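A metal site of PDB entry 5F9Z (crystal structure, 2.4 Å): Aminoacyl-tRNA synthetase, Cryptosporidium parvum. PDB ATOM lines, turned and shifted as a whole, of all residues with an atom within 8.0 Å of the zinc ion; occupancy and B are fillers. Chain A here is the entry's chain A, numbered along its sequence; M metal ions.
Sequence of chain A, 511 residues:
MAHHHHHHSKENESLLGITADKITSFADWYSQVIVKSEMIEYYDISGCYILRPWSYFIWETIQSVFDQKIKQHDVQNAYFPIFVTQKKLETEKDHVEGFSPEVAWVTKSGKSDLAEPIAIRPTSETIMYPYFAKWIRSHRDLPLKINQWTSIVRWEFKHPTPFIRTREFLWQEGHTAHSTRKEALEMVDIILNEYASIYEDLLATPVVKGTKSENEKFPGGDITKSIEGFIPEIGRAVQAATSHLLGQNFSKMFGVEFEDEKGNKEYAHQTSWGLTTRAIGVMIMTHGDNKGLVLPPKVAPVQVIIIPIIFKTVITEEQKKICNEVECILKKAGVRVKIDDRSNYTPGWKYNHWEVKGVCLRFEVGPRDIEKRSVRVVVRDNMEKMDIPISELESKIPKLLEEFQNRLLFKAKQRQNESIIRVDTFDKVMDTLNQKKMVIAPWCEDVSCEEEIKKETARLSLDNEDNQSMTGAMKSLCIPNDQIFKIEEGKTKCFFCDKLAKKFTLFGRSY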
ATOM      1  N   PRO A 442       4.397   4.355 -15.863  1.00  0.00           N
ATOM      2  CA  PRO A 442       3.329   4.008 -14.918  1.00  0.00           C
ATOM      3  C   PRO A 442       2.099   3.534 -15.683  1.00  0.00           C
ATOM      4  O   PRO A 442       1.567   4.253 -16.533  1.00  0.00           O
ATOM      5  CB  PRO A 442       3.064   5.327 -14.179  1.00  0.00           C
ATOM      6  CG  PRO A 442       4.239   6.204 -14.474  1.00  0.00           C
ATOM      7  CD  PRO A 442       4.739   5.785 -15.822  1.00  0.00           C
ATOM      8  N   TRP A 443       1.641   2.328 -15.379  1.00  0.00           N
ATOM      9  CA  TRP A 443       0.578   1.696 -16.148  1.00  0.00           C
ATOM     10  C   TRP A 443      -0.479   1.127 -15.220  1.00  0.00           C
ATOM     11  O   TRP A 443      -0.183   0.660 -14.115  1.00  0.00           O
ATOM     12  CB  TRP A 443       1.129   0.590 -17.052  1.00  0.00           C
ATOM     13  CG  TRP A 443       0.152   0.136 -18.075  1.00  0.00           C
ATOM     14  CD1 TRP A 443      -0.797   0.888 -18.701  1.00  0.00           C
ATOM     15  CD2 TRP A 443       0.018  -1.197 -18.602  1.00  0.00           C
ATOM     16  NE1 TRP A 443      -1.511   0.118 -19.579  1.00  0.00           N
ATOM     17  CE2 TRP A 443      -1.041  -1.165 -19.540  1.00  0.00           C
ATOM     18  CE3 TRP A 443       0.684  -2.405 -18.361  1.00  0.00           C
ATOM     19  CZ2 TRP A 443      -1.442  -2.300 -20.240  1.00  0.00           C
ATOM     20  CZ3 TRP A 443       0.277  -3.519 -19.067  1.00  0.00           C
ATOM     21  CH2 TRP A 443      -0.772  -3.467 -19.994  1.00  0.00           C
ATOM     22  N   CYS A 444      -1.734   1.148 -15.683  1.00  0.00           N
ATOM     23  CA  CYS A 444      -2.857   0.576 -14.958  1.00  0.00           C
ATOM     24  C   CYS A 444      -3.039  -0.908 -15.225  1.00  0.00           C
ATOM     25  O   CYS A 444      -3.771  -1.575 -14.477  1.00  0.00           O
ATOM     26  CB  CYS A 444      -4.148   1.311 -15.302  1.00  0.00           C
ATOM     27  SG  CYS A 444      -4.783   0.953 -16.960  1.00  0.00           S
ATOM     28  N   GLU A 445      -2.422  -1.436 -16.285  1.00  0.00           N
ATOM     29  CA  GLU A 445      -2.411  -2.849 -16.652  1.00  0.00           C
ATOM     30  C   GLU A 445      -3.762  -3.370 -17.112  1.00  0.00           C
ATOM     31  O   GLU A 445      -3.947  -4.592 -17.192  1.00  0.00           O
ATOM     32  CB  GLU A 445      -1.877  -3.727 -15.514  1.00  0.00           C
ATOM     33  CG  GLU A 445      -0.494  -3.329 -15.028  1.00  0.00           C
ATOM     34  CD  GLU A 445      -0.056  -4.122 -13.822  1.00  0.00           C
ATOM     35  OE1 GLU A 445      -0.664  -5.184 -13.541  1.00  0.00           O
ATOM     36  OE2 GLU A 445       0.904  -3.697 -13.142  1.00  0.00           O
ATOM     37  N   ASP A 446      -4.718  -2.496 -17.415  1.00  0.00           N
ATOM     38  CA  ASP A 446      -5.994  -2.951 -17.946  1.00  0.00           C
ATOM     39  C   ASP A 446      -5.845  -3.431 -19.382  1.00  0.00           C
ATOM     40  O   ASP A 446      -5.035  -2.911 -20.152  1.00  0.00           O
ATOM     41  CB  ASP A 446      -7.042  -1.845 -17.878  1.00  0.00           C
ATOM     42  CG  ASP A 446      -7.374  -1.445 -16.450  1.00  0.00           C
ATOM     43  OD1 ASP A 446      -7.111  -2.243 -15.524  1.00  0.00           O
ATOM     44  OD2 ASP A 446      -7.906  -0.330 -16.259  1.00  0.00           O
ATOM     45  N   VAL A 447      -6.649  -4.438 -19.753  1.00  0.00           N
ATOM     46  CA  VAL A 447      -6.651  -4.924 -21.120  1.00  0.00           C
ATOM     47  C   VAL A 447      -7.145  -3.839 -22.069  1.00  0.00           C
ATOM     48  O   VAL A 447      -6.608  -3.662 -23.167  1.00  0.00           O
ATOM     49  CB  VAL A 447      -7.501  -6.205 -21.240  1.00  0.00           C
ATOM     50  CG1 VAL A 447      -7.675  -6.609 -22.697  1.00  0.00           C
ATOM     51  CG2 VAL A 447      -6.883  -7.335 -20.433  1.00  0.00           C
ATOM     52  N   SER A 448      -8.169  -3.086 -21.654  1.00  0.00           N
ATOM     53  CA  SER A 448      -8.698  -2.018 -22.493  1.00  0.00           C
ATOM     54  C   SER A 448      -7.645  -0.935 -22.725  1.00  0.00           C
ATOM     55  O   SER A 448      -7.599  -0.333 -23.812  1.00  0.00           O
ATOM     56  CB  SER A 448      -9.953  -1.427 -21.857  1.00  0.00           C
ATOM     57  OG  SER A 448      -9.698  -1.029 -20.514  1.00  0.00           O
ATOM     58  N   CYS A 449      -6.803  -0.662 -21.727  1.00  0.00           N
ATOM     59  CA  CYS A 449      -5.784   0.360 -21.888  1.00  0.00           C
ATOM     60  C   CYS A 449      -4.724  -0.078 -22.889  1.00  0.00           C
ATOM     61  O   CYS A 449      -4.337   0.704 -23.772  1.00  0.00           O
ATOM     62  CB  CYS A 449      -5.148   0.684 -20.538  1.00  0.00           C
ATOM     63  SG  CYS A 449      -4.082   2.149 -20.548  1.00  0.00           S
ATOM     64  N   GLU A 450      -4.247  -1.321 -22.783  1.00  0.00           N
ATOM     65  CA  GLU A 450      -3.248  -1.801 -23.723  1.00  0.00           C
ATOM     66  C   GLU A 450      -3.800  -1.902 -25.143  1.00  0.00           C
ATOM     67  O   GLU A 450      -3.067  -1.668 -26.104  1.00  0.00           O
ATOM     68  CB  GLU A 450      -2.704  -3.161 -23.278  1.00  0.00           C
ATOM     69  CG  GLU A 450      -1.511  -3.635 -24.088  1.00  0.00           C
ATOM     70  CD  GLU A 450      -0.840  -4.848 -23.496  1.00  0.00           C
ATOM     71  OE1 GLU A 450      -1.376  -5.415 -22.520  1.00  0.00           O
ATOM     72  OE2 GLU A 450       0.237  -5.245 -24.004  1.00  0.00           O
ATOM     73  N   ILE A 453      -3.477   1.501 -26.294  1.00  0.00           N
ATOM     74  CA  ILE A 453      -2.058   1.837 -26.411  1.00  0.00           C
ATOM     75  C   ILE A 453      -1.491   1.296 -27.711  1.00  0.00           C
ATOM     76  O   ILE A 453      -0.807   1.997 -28.462  1.00  0.00           O
ATOM     77  CB  ILE A 453      -1.274   1.313 -25.188  1.00  0.00           C
ATOM     78  CG1 ILE A 453      -1.583   2.156 -23.948  1.00  0.00           C
ATOM     79  CG2 ILE A 453       0.221   1.301 -25.471  1.00  0.00           C
ATOM     80  CD1 ILE A 453      -1.074   1.555 -22.667  1.00  0.00           C
ATOM     81  N   LYS A 493      -1.022   8.279 -11.717  1.00  0.00           N
ATOM     82  CA  LYS A 493      -1.968   7.813 -12.709  1.00  0.00           C
ATOM     83  C   LYS A 493      -1.246   7.066 -13.829  1.00  0.00           C
ATOM     84  O   LYS A 493      -0.022   7.149 -13.978  1.00  0.00           O
ATOM     85  CB  LYS A 493      -2.772   8.972 -13.287  1.00  0.00           C
ATOM     86  N   CYS A 494      -2.029   6.328 -14.612  1.00  0.00           N
ATOM     87  CA  CYS A 494      -1.475   5.644 -15.774  1.00  0.00           C
ATOM     88  C   CYS A 494      -0.929   6.649 -16.767  1.00  0.00           C
ATOM     89  O   CYS A 494      -1.461   7.758 -16.921  1.00  0.00           O
ATOM     90  CB  CYS A 494      -2.557   4.771 -16.429  1.00  0.00           C
ATOM     91  SG  CYS A 494      -2.074   4.067 -18.025  1.00  0.00           S
ATOM     92  N   PHE A 495       0.148   6.266 -17.451  1.00  0.00           N
ATOM     93  CA  PHE A 495       0.752   7.146 -18.447  1.00  0.00           C
ATOM     94  C   PHE A 495      -0.145   7.371 -19.657  1.00  0.00           C
ATOM     95  O   PHE A 495       0.143   8.283 -20.443  1.00  0.00           O
ATOM     96  CB  PHE A 495       2.104   6.578 -18.905  1.00  0.00           C
ATOM     97  CG  PHE A 495       1.981   5.503 -19.948  1.00  0.00           C
ATOM     98  CD1 PHE A 495       1.544   4.230 -19.607  1.00  0.00           C
ATOM     99  CD2 PHE A 495       2.306   5.762 -21.271  1.00  0.00           C
ATOM    100  CE1 PHE A 495       1.443   3.236 -20.569  1.00  0.00           C
ATOM    101  CE2 PHE A 495       2.205   4.768 -22.233  1.00  0.00           C
ATOM    102  CZ  PHE A 495       1.767   3.513 -21.879  1.00  0.00           C
ATOM    103  N   PHE A 496      -1.209   6.589 -19.813  1.00  0.00           N
ATOM    104  CA  PHE A 496      -2.066   6.667 -20.982  1.00  0.00           C
ATOM    105  C   PHE A 496      -3.505   7.035 -20.627  1.00  0.00           C
ATOM    106  O   PHE A 496      -4.045   7.988 -21.199  1.00  0.00           O
ATOM    107  CB  PHE A 496      -2.038   5.322 -21.729  1.00  0.00           C
ATOM    108  CG  PHE A 496      -2.705   5.361 -23.067  1.00  0.00           C
ATOM    109  CD1 PHE A 496      -2.051   5.879 -24.173  1.00  0.00           C
ATOM    110  CD2 PHE A 496      -3.986   4.857 -23.240  1.00  0.00           C
ATOM    111  CE1 PHE A 496      -2.655   5.920 -25.412  1.00  0.00           C
ATOM    112  CE2 PHE A 496      -4.596   4.884 -24.469  1.00  0.00           C
ATOM    113  CZ  PHE A 496      -3.941   5.410 -25.564  1.00  0.00           C
ATOM    114  N   CYS A 497      -4.136   6.301 -19.716  1.00  0.00           N
ATOM    115  CA  CYS A 497      -5.526   6.550 -19.350  1.00  0.00           C
ATOM    116  C   CYS A 497      -5.601   7.244 -17.994  1.00  0.00           C
ATOM    117  O   CYS A 497      -4.583   7.543 -17.359  1.00  0.00           O
ATOM    118  CB  CYS A 497      -6.324   5.245 -19.351  1.00  0.00           C
ATOM    119  SG  CYS A 497      -6.087   4.243 -17.876  1.00  0.00           S
ATOM    120  N   ASP A 498      -6.821   7.506 -17.553  1.00  0.00           N
ATOM    121  CA  ASP A 498      -7.069   8.247 -16.323  1.00  0.00           C
ATOM    122  C   ASP A 498      -7.086   7.372 -15.078  1.00  0.00           C
ATOM    123  O   ASP A 498      -7.338   7.882 -13.987  1.00  0.00           O
ATOM    124  CB  ASP A 498      -8.406   9.009 -16.422  1.00  0.00           C
ATOM    125  N   LYS A 499      -6.828   6.078 -15.207  1.00  0.00           N
ATOM    126  CA  LYS A 499      -6.840   5.189 -14.048  1.00  0.00           C
ATOM    127  C   LYS A 499      -5.536   5.311 -13.273  1.00  0.00           C
ATOM    128  O   LYS A 499      -4.509   5.764 -13.784  1.00  0.00           O
ATOM    129  CB  LYS A 499      -7.056   3.742 -14.478  1.00  0.00           C
ATOM    130  N   LEU A 500      -5.592   4.901 -12.008  1.00  0.00           N
ATOM    131  CA  LEU A 500      -4.408   4.927 -11.155  1.00  0.00           C
ATOM    132  C   LEU A 500      -3.426   3.850 -11.589  1.00  0.00           C
ATOM    133  O   LEU A 500      -3.815   2.722 -11.895  1.00  0.00           O
ATOM    134  CB  LEU A 500      -4.798   4.732  -9.690  1.00  0.00           C
ATOM    135  N   ALA A 501      -2.141   4.194 -11.598  1.00  0.00           N
ATOM    136  CA  ALA A 501      -1.110   3.256 -12.012  1.00  0.00           C
ATOM    137  C   ALA A 501      -0.870   2.227 -10.928  1.00  0.00           C
ATOM    138  O   ALA A 501      -0.753   2.563  -9.748  1.00  0.00           O
ATOM    139  CB  ALA A 501       0.181   3.994 -12.337  1.00  0.00           C
ATOM    140  N   LYS A 502      -0.811   0.953 -11.327  1.00  0.00           N
ATOM    141  CA  LYS A 502      -0.526  -0.117 -10.365  1.00  0.00           C
ATOM    142  C   LYS A 502       0.972  -0.259 -10.137  1.00  0.00           C
ATOM    143  O   LYS A 502       1.438  -0.232  -8.989  1.00  0.00           O
ATOM    144  CB  LYS A 502      -1.125  -1.439 -10.856  1.00  0.00           C
ATOM    145  CG  LYS A 502      -2.641  -1.486 -10.764  1.00  0.00           C
ATOM    146  CD  LYS A 502      -3.193  -2.799 -11.318  1.00  0.00           C
ATOM    147  CE  LYS A 502      -4.650  -2.975 -10.938  1.00  0.00           C
ATOM    148  NZ  LYS A 502      -5.477  -1.805 -11.331  1.00  0.00           N
ATOM    149  N   PHE A 507       7.482  -1.217 -21.908  1.00  0.00           N
ATOM    150  CA  PHE A 507       6.811  -1.157 -23.200  1.00  0.00           C
ATOM    151  C   PHE A 507       7.839  -1.068 -24.330  1.00  0.00           C
ATOM    152  O   PHE A 507       9.007  -0.725 -24.112  1.00  0.00           O
ATOM    153  CB  PHE A 507       5.860   0.035 -23.277  1.00  0.00           C
ATOM    154  CG  PHE A 507       4.610  -0.130 -22.468  1.00  0.00           C
ATOM    155  CD1 PHE A 507       4.568   0.265 -21.145  1.00  0.00           C
ATOM    156  CD2 PHE A 507       3.468  -0.669 -23.035  1.00  0.00           C
ATOM    157  CE1 PHE A 507       3.415   0.118 -20.399  1.00  0.00           C
ATOM    158  CE2 PHE A 507       2.312  -0.815 -22.299  1.00  0.00           C
ATOM    159  CZ  PHE A 507       2.281  -0.417 -20.978  1.00  0.00           C
HETATM  160 ZN    ZN M   1      -4.179   2.736 -18.296  1.00  0.00          ZN
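The side-chain carboxylate (OD2) of Asp 446 lies close to the side-chain sulfur (SG) of Cys 444, 3.4 Å away. The backbone NH of Cys 494 lies within hydrogen-bond range of the backbone carbonyl oxygen of Lys 499 (2.7 Å). SG of Cys 494 lies close to N of Phe 496 (3.2 Å). N of Lys 499 sits close to SG of Cys 497 (3.3 Å). The indole nitrogen of Trp 443 lies close to the side-chain sulfur of Cys 449 (3.4 Å). The backbone carbonyl oxygen of Trp 443 sits at hydrogen-bond distance from the backbone NH of Lys 502 (2.9 Å).
CD1 of Trp 443 touches the zinc ion (3.9 Å). Within 4 Å of the zinc ion: Trp 443, Cys 444, Cys 449, Cys 494 and Cys 497.
The zinc ion is bound by the side-chain sulfur (SG) of Cys 444, at 2.3 Å. SG of Cys 449 is bound to the zinc ion, 2.3 Å away. SG of Cys 497 is bound to the zinc ion (2.5 Å). The zinc ion is bound by the side-chain sulfur (SG) of Cys 494. The zinc ion has four donor atoms within binding distance.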
